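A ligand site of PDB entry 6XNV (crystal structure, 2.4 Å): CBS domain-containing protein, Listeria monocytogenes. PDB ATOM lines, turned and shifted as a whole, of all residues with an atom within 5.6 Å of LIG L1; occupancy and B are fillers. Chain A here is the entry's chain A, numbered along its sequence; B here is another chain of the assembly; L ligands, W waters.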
ATOM      1  N   ILE A  32      -4.454  21.584  -1.692  1.00  0.00           N
ATOM      2  CA  ILE A  32      -3.846  22.574  -2.583  1.00  0.00           C
ATOM      3  C   ILE A  32      -2.827  21.866  -3.450  1.00  0.00           C
ATOM      4  O   ILE A  32      -1.835  21.328  -2.940  1.00  0.00           O
ATOM      5  CB  ILE A  32      -3.188  23.722  -1.799  1.00  0.00           C
ATOM      6  CG1 ILE A  32      -4.039  24.140  -0.591  1.00  0.00           C
ATOM      7  CG2 ILE A  32      -2.876  24.887  -2.711  1.00  0.00           C
ATOM      8  CD1 ILE A  32      -5.207  25.076  -0.935  1.00  0.00           C
ATOM      9  N   LYS A  36       0.501  25.119  -7.059  1.00  0.00           N
ATOM     10  CA  LYS A  36       0.059  26.355  -6.429  1.00  0.00           C
ATOM     11  C   LYS A  36       0.813  26.676  -5.148  1.00  0.00           C
ATOM     12  O   LYS A  36       0.545  27.708  -4.525  1.00  0.00           O
ATOM     13  CB  LYS A  36      -1.440  26.274  -6.140  1.00  0.00           C
ATOM     14  CG  LYS A  36      -2.258  25.814  -7.353  1.00  0.00           C
ATOM     15  CD  LYS A  36      -3.768  25.871  -7.073  1.00  0.00           C
ATOM     16  CE  LYS A  36      -4.427  27.008  -7.843  1.00  0.00           C
ATOM     17  NZ  LYS A  36      -3.668  28.267  -7.673  1.00  0.00           N
ATOM     18  N   VAL A  37       1.784  25.845  -4.747  1.00  0.00           N
ATOM     19  CA  VAL A  37       2.452  25.939  -3.454  1.00  0.00           C
ATOM     20  C   VAL A  37       3.841  26.505  -3.697  1.00  0.00           C
ATOM     21  O   VAL A  37       4.644  25.905  -4.432  1.00  0.00           O
ATOM     22  CB  VAL A  37       2.551  24.567  -2.777  1.00  0.00           C
ATOM     23  CG1 VAL A  37       3.542  24.603  -1.599  1.00  0.00           C
ATOM     24  CG2 VAL A  37       1.188  24.072  -2.342  1.00  0.00           C
ATOM     25  N   ALA A  38       4.136  27.652  -3.084  1.00  0.00           N
ATOM     26  CA  ALA A  38       5.493  28.188  -3.139  1.00  0.00           C
ATOM     27  C   ALA A  38       6.445  27.302  -2.341  1.00  0.00           C
ATOM     28  O   ALA A  38       6.076  26.734  -1.310  1.00  0.00           O
ATOM     29  CB  ALA A  38       5.535  29.614  -2.591  1.00  0.00           C
ATOM     30  N   CYS A  56       6.654  35.553  -1.931  1.00  0.00           N
ATOM     31  CA  CYS A  56       5.400  34.800  -2.021  1.00  0.00           C
ATOM     32  C   CYS A  56       4.419  35.113  -0.909  1.00  0.00           C
ATOM     33  O   CYS A  56       3.279  34.709  -1.020  1.00  0.00           O
ATOM     34  CB  CYS A  56       5.612  33.285  -2.034  1.00  0.00           C
ATOM     35  SG  CYS A  56       6.096  32.567  -0.409  1.00  0.00           S
ATOM     36  N   GLY A  57       4.823  35.779   0.174  1.00  0.00           N
ATOM     37  CA  GLY A  57       3.880  36.128   1.201  1.00  0.00           C
ATOM     38  C   GLY A  57       3.519  35.048   2.212  1.00  0.00           C
ATOM     39  O   GLY A  57       2.782  35.345   3.162  1.00  0.00           O
ATOM     40  N   TYR A  58       3.979  33.809   2.031  1.00  0.00           N
ATOM     41  CA  TYR A  58       3.717  32.767   3.025  1.00  0.00           C
ATOM     42  C   TYR A  58       4.880  32.667   3.998  1.00  0.00           C
ATOM     43  O   TYR A  58       6.046  32.819   3.608  1.00  0.00           O
ATOM     44  CB  TYR A  58       3.495  31.428   2.346  1.00  0.00           C
ATOM     45  CG  TYR A  58       2.275  31.466   1.512  1.00  0.00           C
ATOM     46  CD1 TYR A  58       1.016  31.589   2.117  1.00  0.00           C
ATOM     47  CD2 TYR A  58       2.338  31.412   0.124  1.00  0.00           C
ATOM     48  CE1 TYR A  58      -0.122  31.644   1.349  1.00  0.00           C
ATOM     49  CE2 TYR A  58       1.189  31.454  -0.654  1.00  0.00           C
ATOM     50  CZ  TYR A  58      -0.030  31.565  -0.019  1.00  0.00           C
ATOM     51  OH  TYR A  58      -1.186  31.611  -0.757  1.00  0.00           O
ATOM     52  N   SER A  59       4.570  32.402   5.260  1.00  0.00           N
ATOM     53  CA  SER A  59       5.588  32.455   6.290  1.00  0.00           C
ATOM     54  C   SER A  59       6.283  31.115   6.545  1.00  0.00           C
ATOM     55  O   SER A  59       7.329  31.113   7.210  1.00  0.00           O
ATOM     56  CB  SER A  59       4.977  32.969   7.583  1.00  0.00           C
ATOM     57  OG  SER A  59       3.850  32.193   7.908  1.00  0.00           O
ATOM     58  N   VAL A  60       5.748  29.991   6.062  1.00  0.00           N
ATOM     59  CA  VAL A  60       6.385  28.668   6.165  1.00  0.00           C
ATOM     60  C   VAL A  60       6.102  27.929   4.870  1.00  0.00           C
ATOM     61  O   VAL A  60       4.934  27.799   4.463  1.00  0.00           O
ATOM     62  CB  VAL A  60       5.854  27.836   7.353  1.00  0.00           C
ATOM     63  CG1 VAL A  60       6.566  26.472   7.429  1.00  0.00           C
ATOM     64  CG2 VAL A  60       5.954  28.572   8.712  1.00  0.00           C
ATOM     65  N   ILE A  61       7.149  27.409   4.220  1.00  0.00           N
ATOM     66  CA  ILE A  61       6.969  26.766   2.927  1.00  0.00           C
ATOM     67  C   ILE A  61       7.876  25.548   2.822  1.00  0.00           C
ATOM     68  O   ILE A  61       8.887  25.436   3.527  1.00  0.00           O
ATOM     69  CB  ILE A  61       7.235  27.724   1.745  1.00  0.00           C
ATOM     70  CG1 ILE A  61       8.697  28.174   1.744  1.00  0.00           C
ATOM     71  CG2 ILE A  61       6.245  28.890   1.732  1.00  0.00           C
ATOM     72  CD1 ILE A  61       9.017  28.988   0.532  1.00  0.00           C
ATOM     73  N   PRO A  62       7.545  24.604   1.934  1.00  0.00           N
ATOM     74  CA  PRO A  62       8.368  23.410   1.792  1.00  0.00           C
ATOM     75  C   PRO A  62       9.678  23.680   1.061  1.00  0.00           C
ATOM     76  O   PRO A  62       9.858  24.660   0.329  1.00  0.00           O
ATOM     77  CB  PRO A  62       7.488  22.446   1.011  1.00  0.00           C
ATOM     78  CG  PRO A  62       6.430  23.244   0.418  1.00  0.00           C
ATOM     79  CD  PRO A  62       6.221  24.421   1.316  1.00  0.00           C
ATOM     80  N   PRO A 127      -0.316  24.450  11.007  1.00  0.00           N
ATOM     81  CA  PRO A 127      -1.164  25.207  10.068  1.00  0.00           C
ATOM     82  C   PRO A 127      -1.363  24.521   8.754  1.00  0.00           C
ATOM     83  O   PRO A 127      -2.323  24.839   8.043  1.00  0.00           O
ATOM     84  CB  PRO A 127      -0.410  26.534   9.888  1.00  0.00           C
ATOM     85  CG  PRO A 127       0.427  26.664  11.130  1.00  0.00           C
ATOM     86  CD  PRO A 127       0.849  25.232  11.465  1.00  0.00           C
ATOM     87  N   PHE A 128      -0.481  23.601   8.358  1.00  0.00           N
ATOM     88  CA  PHE A 128      -0.656  22.829   7.144  1.00  0.00           C
ATOM     89  C   PHE A 128       0.202  21.578   7.250  1.00  0.00           C
ATOM     90  O   PHE A 128       1.180  21.548   8.003  1.00  0.00           O
ATOM     91  CB  PHE A 128      -0.263  23.625   5.897  1.00  0.00           C
ATOM     92  CG  PHE A 128       1.243  23.793   5.724  1.00  0.00           C
ATOM     93  CD1 PHE A 128       1.911  24.864   6.324  1.00  0.00           C
ATOM     94  CD2 PHE A 128       1.976  22.880   4.976  1.00  0.00           C
ATOM     95  CE1 PHE A 128       3.273  25.029   6.154  1.00  0.00           C
ATOM     96  CE2 PHE A 128       3.350  23.023   4.839  1.00  0.00           C
ATOM     97  CZ  PHE A 128       4.000  24.103   5.408  1.00  0.00           C
ATOM     98  N   ILE A 141      -0.615  20.267  -0.258  1.00  0.00           N
ATOM     99  CA  ILE A 141      -0.779  20.481   1.170  1.00  0.00           C
ATOM    100  C   ILE A 141      -2.254  20.530   1.558  1.00  0.00           C
ATOM    101  O   ILE A 141      -3.137  20.738   0.731  1.00  0.00           O
ATOM    102  CB  ILE A 141      -0.057  21.771   1.650  1.00  0.00           C
ATOM    103  CG1 ILE A 141      -0.792  23.010   1.141  1.00  0.00           C
ATOM    104  CG2 ILE A 141       1.449  21.762   1.218  1.00  0.00           C
ATOM    105  CD1 ILE A 141      -0.168  24.334   1.566  1.00  0.00           C
ATOM    106  N   THR A 143      -4.503  22.535   4.451  1.00  0.00           N
ATOM    107  CA  THR A 143      -4.360  23.668   5.359  1.00  0.00           C
ATOM    108  C   THR A 143      -5.516  23.731   6.336  1.00  0.00           C
ATOM    109  O   THR A 143      -6.584  23.146   6.106  1.00  0.00           O
ATOM    110  CB  THR A 143      -4.296  24.976   4.568  1.00  0.00           C
ATOM    111  OG1 THR A 143      -5.522  25.146   3.845  1.00  0.00           O
ATOM    112  CG2 THR A 143      -3.105  24.977   3.590  1.00  0.00           C
ATOM    113  N   ARG A 144      -5.274  24.426   7.458  1.00  0.00           N
ATOM    114  CA  ARG A 144      -6.339  24.694   8.407  1.00  0.00           C
ATOM    115  C   ARG A 144      -7.505  25.373   7.731  1.00  0.00           C
ATOM    116  O   ARG A 144      -8.672  25.116   8.080  1.00  0.00           O
ATOM    117  CB  ARG A 144      -5.861  25.614   9.535  1.00  0.00           C
ATOM    118  CG  ARG A 144      -5.036  24.964  10.578  1.00  0.00           C
ATOM    119  CD  ARG A 144      -4.384  25.994  11.459  1.00  0.00           C
ATOM    120  NE  ARG A 144      -3.791  25.332  12.607  1.00  0.00           N
ATOM    121  CZ  ARG A 144      -3.196  25.956  13.618  1.00  0.00           C
ATOM    122  NH1 ARG A 144      -2.719  25.245  14.623  1.00  0.00           N
ATOM    123  NH2 ARG A 144      -3.115  27.291  13.624  1.00  0.00           N
ATOM    124  N   ARG A 145      -7.228  26.236   6.754  1.00  0.00           N
ATOM    125  CA  ARG A 145      -8.271  27.002   6.087  1.00  0.00           C
ATOM    126  C   ARG A 145      -9.393  26.117   5.541  1.00  0.00           C
ATOM    127  O   ARG A 145     -10.572  26.475   5.650  1.00  0.00           O
ATOM    128  CB  ARG A 145      -7.649  27.857   4.984  1.00  0.00           C
ATOM    129  CG  ARG A 145      -8.582  28.952   4.482  1.00  0.00           C
ATOM    130  CD  ARG A 145      -7.877  29.909   3.547  1.00  0.00           C
ATOM    131  NE  ARG A 145      -8.739  31.046   3.243  1.00  0.00           N
ATOM    132  CZ  ARG A 145      -9.666  31.039   2.290  1.00  0.00           C
ATOM    133  NH1 ARG A 145      -9.855  29.956   1.542  1.00  0.00           N
ATOM    134  NH2 ARG A 145     -10.407  32.139   2.077  1.00  0.00           N
ATOM    135  N   VAL A 146      -9.057  24.954   4.973  1.00  0.00           N
ATOM    136  CA  VAL A 146     -10.112  24.095   4.438  1.00  0.00           C
ATOM    137  C   VAL A 146     -10.987  23.508   5.529  1.00  0.00           C
ATOM    138  O   VAL A 146     -12.184  23.267   5.313  1.00  0.00           O
ATOM    139  CB  VAL A 146      -9.568  22.959   3.575  1.00  0.00           C
ATOM    140  CG1 VAL A 146     -10.769  22.463   2.816  1.00  0.00           C
ATOM    141  CG2 VAL A 146      -8.454  23.490   2.666  1.00  0.00           C
ATOM    142  N   SER B  59       4.974  34.320  14.003  1.00  0.00           N
ATOM    143  CA  SER B  59       5.212  34.931  12.710  1.00  0.00           C
ATOM    144  C   SER B  59       4.536  36.290  12.545  1.00  0.00           C
ATOM    145  O   SER B  59       5.030  37.122  11.780  1.00  0.00           O
ATOM    146  CB  SER B  59       4.765  34.009  11.570  1.00  0.00           C
ATOM    147  OG  SER B  59       3.389  33.738  11.697  1.00  0.00           O
ATOM    148  N   VAL B 124     -11.387  32.013   9.179  1.00  0.00           N
ATOM    149  CA  VAL B 124     -11.165  31.293   7.923  1.00  0.00           C
ATOM    150  C   VAL B 124     -10.012  31.915   7.147  1.00  0.00           C
ATOM    151  O   VAL B 124      -9.328  31.228   6.378  1.00  0.00           O
ATOM    152  CB  VAL B 124     -12.454  31.280   7.072  1.00  0.00           C
ATOM    153  CG1 VAL B 124     -12.176  30.820   5.640  1.00  0.00           C
ATOM    154  CG2 VAL B 124     -13.526  30.403   7.736  1.00  0.00           C
ATOM    155  N   ASP B 125      -9.776  33.211   7.306  1.00  0.00           N
ATOM    156  CA  ASP B 125      -8.765  33.883   6.523  1.00  0.00           C
ATOM    157  C   ASP B 125      -7.725  34.589   7.381  1.00  0.00           C
ATOM    158  O   ASP B 125      -6.791  35.183   6.835  1.00  0.00           O
ATOM    159  CB  ASP B 125      -9.426  34.888   5.554  1.00  0.00           C
ATOM    160  CG  ASP B 125      -9.983  34.221   4.287  1.00  0.00           C
ATOM    161  OD1 ASP B 125     -11.172  33.791   4.279  1.00  0.00           O
ATOM    162  OD2 ASP B 125      -9.237  34.124   3.288  1.00  0.00           O
ATOM    163  N   HIS B 126      -7.847  34.519   8.698  1.00  0.00           N
ATOM    164  CA  HIS B 126      -6.900  35.182   9.594  1.00  0.00           C
ATOM    165  C   HIS B 126      -6.476  34.223  10.698  1.00  0.00           C
ATOM    166  O   HIS B 126      -7.334  33.765  11.475  1.00  0.00           O
ATOM    167  CB  HIS B 126      -7.514  36.463  10.175  1.00  0.00           C
ATOM    168  CG  HIS B 126      -7.839  37.476   9.129  1.00  0.00           C
ATOM    169  ND1 HIS B 126      -8.852  37.311   8.216  1.00  0.00           N
ATOM    170  CD2 HIS B 126      -7.240  38.655   8.818  1.00  0.00           C
ATOM    171  CE1 HIS B 126      -8.885  38.350   7.404  1.00  0.00           C
ATOM    172  NE2 HIS B 126      -7.919  39.175   7.747  1.00  0.00           N
ATOM    173  N   PRO B 127      -5.193  33.912  10.805  1.00  0.00           N
ATOM    174  CA  PRO B 127      -4.747  32.998  11.869  1.00  0.00           C
ATOM    175  C   PRO B 127      -5.246  33.393  13.253  1.00  0.00           C
ATOM    176  O   PRO B 127      -5.582  32.518  14.056  1.00  0.00           O
ATOM    177  CB  PRO B 127      -3.212  33.076  11.779  1.00  0.00           C
ATOM    178  CG  PRO B 127      -2.952  33.423  10.389  1.00  0.00           C
ATOM    179  CD  PRO B 127      -4.077  34.297   9.924  1.00  0.00           C
ATOM    180  N   ARG B 144      -6.948  30.473  15.618  1.00  0.00           N
ATOM    181  CA  ARG B 144      -7.497  29.303  14.937  1.00  0.00           C
ATOM    182  C   ARG B 144      -7.392  28.058  15.798  1.00  0.00           C
ATOM    183  O   ARG B 144      -8.302  27.213  15.805  1.00  0.00           O
ATOM    184  CB  ARG B 144      -6.762  29.081  13.607  1.00  0.00           C
ATOM    185  CG  ARG B 144      -7.029  30.102  12.508  1.00  0.00           C
ATOM    186  CD  ARG B 144      -6.187  29.766  11.284  1.00  0.00           C
ATOM    187  NE  ARG B 144      -6.644  30.418  10.061  1.00  0.00           N
ATOM    188  CZ  ARG B 144      -6.045  30.326   8.883  1.00  0.00           C
ATOM    189  NH1 ARG B 144      -6.567  30.944   7.831  1.00  0.00           N
ATOM    190  NH2 ARG B 144      -4.920  29.606   8.750  1.00  0.00           N
HETATM  191  P1  LIG L   1      -3.983  28.834   5.390  1.00  0.00           P
HETATM  192  O1  LIG L   1      -4.489  28.998   3.985  1.00  0.00           O
HETATM  193  O2  LIG L   1      -4.597  27.785   6.285  1.00  0.00           O
HETATM  194  O3  LIG L   1      -2.391  28.500   5.294  1.00  0.00           O
HETATM  195  C1  LIG L   1      -1.734  27.866   6.378  1.00  0.00           C
HETATM  196  C2  LIG L   1      -0.233  27.899   6.167  1.00  0.00           C
HETATM  197  O4  LIG L   1       0.102  26.964   5.119  1.00  0.00           O
HETATM  198  C3  LIG L   1       0.280  29.244   5.663  1.00  0.00           C
HETATM  199  O5  LIG L   1       0.593  30.083   6.759  1.00  0.00           O
HETATM  200  C4  LIG L   1       1.516  28.840   4.896  1.00  0.00           C
HETATM  201  O6  LIG L   1       2.606  28.474   5.741  1.00  0.00           O
HETATM  202  C5  LIG L   1       1.128  27.516   4.296  1.00  0.00           C
HETATM  203  N1  LIG L   1       0.574  27.749   2.953  1.00  0.00           N
HETATM  204  C6  LIG L   1      -0.726  27.844   2.634  1.00  0.00           C
HETATM  205  N2  LIG L   1      -0.889  28.061   1.299  1.00  0.00           N
HETATM  206  C7  LIG L   1       0.332  28.089   0.756  1.00  0.00           C
HETATM  207  C8  LIG L   1       0.880  28.261  -0.601  1.00  0.00           C
HETATM  208  N3  LIG L   1       0.097  28.451  -1.687  1.00  0.00           N
HETATM  209  N4  LIG L   1       2.232  28.220  -0.714  1.00  0.00           N
HETATM  210  C9  LIG L   1       3.041  28.039   0.330  1.00  0.00           C
HETATM  211  N5  LIG L   1       2.609  27.879   1.590  1.00  0.00           N
HETATM  212  C10 LIG L   1       1.287  27.893   1.859  1.00  0.00           C
HETATM  213  P2  LIG L   1       0.764  31.672   6.659  1.00  0.00           P
HETATM  214  O7  LIG L   1       1.638  32.085   5.499  1.00  0.00           O
HETATM  215  O8  LIG L   1       1.082  32.035   8.062  1.00  0.00           O
HETATM  216  O9  LIG L   1      -0.761  32.068   6.316  1.00  0.00           O
HETATM  217  C11 LIG L   1      -1.738  32.108   7.361  1.00  0.00           C
HETATM  218  C12 LIG L   1      -3.113  32.384   6.760  1.00  0.00           C
HETATM  219  O10 LIG L   1      -3.171  33.679   6.115  1.00  0.00           O
HETATM  220  C13 LIG L   1      -3.454  31.395   5.649  1.00  0.00           C
HETATM  221  O11 LIG L   1      -4.004  30.208   6.207  1.00  0.00           O
HETATM  222  C14 LIG L   1      -4.414  32.170   4.768  1.00  0.00           C
HETATM  223  O12 LIG L   1      -5.773  31.874   5.178  1.00  0.00           O
HETATM  224  C15 LIG L   1      -4.047  33.635   4.999  1.00  0.00           C
HETATM  225  N6  LIG L   1      -3.300  34.020   3.798  1.00  0.00           N
HETATM  226  C16 LIG L   1      -1.982  34.218   3.689  1.00  0.00           C
HETATM  227  N7  LIG L   1      -1.667  34.502   2.379  1.00  0.00           N
HETATM  228  C17 LIG L   1      -2.795  34.482   1.655  1.00  0.00           C
HETATM  229  C18 LIG L   1      -3.203  34.672   0.250  1.00  0.00           C
HETATM  230  N8  LIG L   1      -2.330  34.983  -0.723  1.00  0.00           N
HETATM  231  N9  LIG L   1      -4.516  34.544  -0.063  1.00  0.00           N
HETATM  232  C19 LIG L   1      -5.437  34.226   0.854  1.00  0.00           C
HETATM  233  N10 LIG L   1      -5.136  34.047   2.149  1.00  0.00           N
HETATM  234  C20 LIG L   1      -3.864  34.155   2.607  1.00  0.00           C
HETATM  235  P1  LG2 L   2       2.055  31.615  13.727  1.00  0.00           P
HETATM  236  O1  LG2 L   2       2.183  31.432  12.220  1.00  0.00           O
HETATM  237  O2  LG2 L   2       3.137  32.263  14.557  1.00  0.00           O
HETATM  238  O3  LG2 L   2       1.762  30.165  14.401  1.00  0.00           O
HETATM  239  C1  LG2 L   2       1.075  29.181  13.652  1.00  0.00           C
HETATM  240  C2  LG2 L   2       0.752  27.974  14.533  1.00  0.00           C
HETATM  241  O4  LG2 L   2       1.919  27.235  14.938  1.00  0.00           O
HETATM  242  C3  LG2 L   2       0.060  28.343  15.826  1.00  0.00           C
HETATM  243  O5  LG2 L   2      -1.330  28.477  15.593  1.00  0.00           O
HETATM  244  C4  LG2 L   2       0.377  27.162  16.707  1.00  0.00           C
HETATM  245  O6  LG2 L   2      -0.605  26.153  16.438  1.00  0.00           O
HETATM  246  C5  LG2 L   2       1.748  26.691  16.248  1.00  0.00           C
HETATM  247  N1  LG2 L   2       2.729  27.348  17.116  1.00  0.00           N
HETATM  248  C6  LG2 L   2       3.475  28.414  16.753  1.00  0.00           C
HETATM  249  N2  LG2 L   2       4.256  28.825  17.776  1.00  0.00           N
HETATM  250  C7  LG2 L   2       4.017  28.030  18.820  1.00  0.00           C
HETATM  251  C8  LG2 L   2       4.522  27.930  20.222  1.00  0.00           C
HETATM  252  N3  LG2 L   2       5.451  28.784  20.684  1.00  0.00           N
HETATM  253  N4  LG2 L   2       4.002  26.954  21.002  1.00  0.00           N
HETATM  254  C9  LG2 L   2       3.058  26.093  20.545  1.00  0.00           C
HETATM  255  N5  LG2 L   2       2.561  26.128  19.295  1.00  0.00           N
HETATM  256  C10 LG2 L   2       2.998  27.059  18.389  1.00  0.00           C
HETATM  257  P2  LG2 L   2      -2.260  29.324  16.594  1.00  0.00           P
HETATM  258  O7  LG2 L   2      -1.897  28.941  18.003  1.00  0.00           O
HETATM  259  O8  LG2 L   2      -3.681  29.201  16.043  1.00  0.00           O
HETATM  260  O9  LG2 L   2      -1.773  30.841  16.382  1.00  0.00           O
HETATM  261  C11 LG2 L   2      -2.286  31.618  15.312  1.00  0.00           C
HETATM  262  C12 LG2 L   2      -1.407  32.851  15.156  1.00  0.00           C
HETATM  263  O10 LG2 L   2      -1.682  33.754  16.220  1.00  0.00           O
HETATM  264  C13 LG2 L   2       0.080  32.552  15.245  1.00  0.00           C
HETATM  265  O11 LG2 L   2       0.659  32.407  13.963  1.00  0.00           O
HETATM  266  C14 LG2 L   2       0.640  33.800  15.872  1.00  0.00           C
HETATM  267  O12 LG2 L   2       1.023  34.702  14.829  1.00  0.00           O
HETATM  268  C15 LG2 L   2      -0.494  34.399  16.690  1.00  0.00           C
HETATM  269  N6  LG2 L   2      -0.282  34.036  18.117  1.00  0.00           N
HETATM  270  C16 LG2 L   2      -0.698  32.925  18.726  1.00  0.00           C
HETATM  271  N7  LG2 L   2      -0.303  32.887  20.032  1.00  0.00           N
HETATM  272  C17 LG2 L   2       0.407  34.009  20.272  1.00  0.00           C
HETATM  273  C18 LG2 L   2       1.088  34.626  21.433  1.00  0.00           C
HETATM  274  N8  LG2 L   2       1.150  34.052  22.669  1.00  0.00           N
HETATM  275  N9  LG2 L   2       1.676  35.819  21.232  1.00  0.00           N
HETATM  276  C19 LG2 L   2       1.645  36.444  20.035  1.00  0.00           C
HETATM  277  N10 LG2 L   2       1.039  35.942  18.939  1.00  0.00           N
HETATM  278  C20 LG2 L   2       0.414  34.757  18.994  1.00  0.00           C
HETATM  279  O   HOH W   1      -5.457  27.246   2.383  1.00  0.00           O
HETATM  280  O   HOH W   2       1.042  34.715   5.266  1.00  0.00           O
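An oxygen (O2) of LIG L1 lies within salt-bridge range of the guanidinium group (NH2) of Arg 144 of chain B (3.1 Å). An oxygen (O8) of LG2 L2 is in salt-bridge range of the guanidinium group (NH2) of Arg 144 of chain A, at 3.1 Å. The side-chain hydroxyl of Ser 59 of chain B is in hydrogen-bond range of an oxygen (O1) of LG2 L2 (2.7 Å). An oxygen (O6) of LIG L1 is in hydrogen-bond range of the backbone carbonyl oxygen (O) of Val 60 (2.7 Å). The backbone NH of Ala 38 lies within hydrogen-bond range of a nitrogen (N4) of LIG L1, 3.1 Å away. The backbone NH (N) of Arg 145 lies within hydrogen-bond range of an oxygen (O2) of LIG L1 (3.1 Å). An oxygen (O7) of LIG L1 is in hydrogen-bond range of the backbone NH of Ser 59 of chain A. N of Ser 59 of chain B sits at hydrogen-bond distance from O2 of LG2 L2, 2.8 Å away. An oxygen (O8) of LIG L1 sits at hydrogen-bond distance from the side-chain hydroxyl (OG) of Ser 59 of chain A (2.8 Å). A nitrogen (N3) of LIG L1 is in hydrogen-bond range of the backbone carbonyl oxygen of Lys 36 (3.0 Å).
The guanidinium group (NH1) of Arg 144 of chain B is in hydrogen-bond range of the backbone carbonyl oxygen (O) of Val 124 of chain B (3.1 Å). The backbone NH of Ile 32 sits at hydrogen-bond distance from the backbone carbonyl oxygen of Ile 141 (2.9 Å). The backbone carbonyl oxygen (O) of Val 124 of chain B sits close to the guanidinium group (NE) of Arg 145 (3.2 Å). The backbone NH (N) of Arg 144 of chain B is in hydrogen-bond range of the backbone carbonyl oxygen (O) of Pro 127 of chain B (2.9 Å). The backbone carbonyl oxygen of Pro 127 of chain A sits at hydrogen-bond distance from the backbone NH of Arg 144 of chain A, at 3.0 Å. The side-chain sulfur (SG) of Cys 56 lies close to the backbone NH (N) of Tyr 58, 3.5 Å away. The side-chain carboxylate of Asp 125 of chain B is in salt-bridge range of the guanidinium group of Arg 145.
Val 37 touches LIG L1 (CA to N4, 3.6 Å). CE2 of Tyr 58 touches C8 of LIG L1, 3.2 Å away. CG2 of Ile 61 touches C9 of LIG L1, at 3.6 Å. O of Pro 127 of chain A touches C1 of LIG L1, 3.5 Å away. Phe 128 touches LIG L1 (CD1 to O4, 3.0 Å). Ile 141 touches LIG L1. Thr 143 touches LIG L1 (CB to O2, 3.3 Å). Arg 144 of chain A touches LIG L1 (N to O2, 3.6 Å). Val 124 of chain B touches LIG L1. O of Asp 125 of chain B touches C15 of LIG L1, 3.6 Å away. CG of Pro 127 of chain B touches C11 of LIG L1, at 3.5 Å. Hydrophobic or aromatic side chains within 4 Å of LIG L1: Val 37, Tyr 58, Val 60, Ile 61, Pro 127 of chain A, Phe 128, Ile 141 and Pro 127 of chain B. Of the 24 residues printed, 17 come within 4 Å of LIG L1. The nearest printed residue that does not touch LIG L1 is Gly 57 (4.2 Å).
Water W1 lies within hydrogen-bond range of the side-chain hydroxyl (OG1) of Thr 143 and an oxygen (O1) of LIG L1. Water W2 lies within hydrogen-bond range of an oxygen (O7) of LIG L1 (2.7 Å) and the backbone carbonyl oxygen of Gly 57 (2.8 Å).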
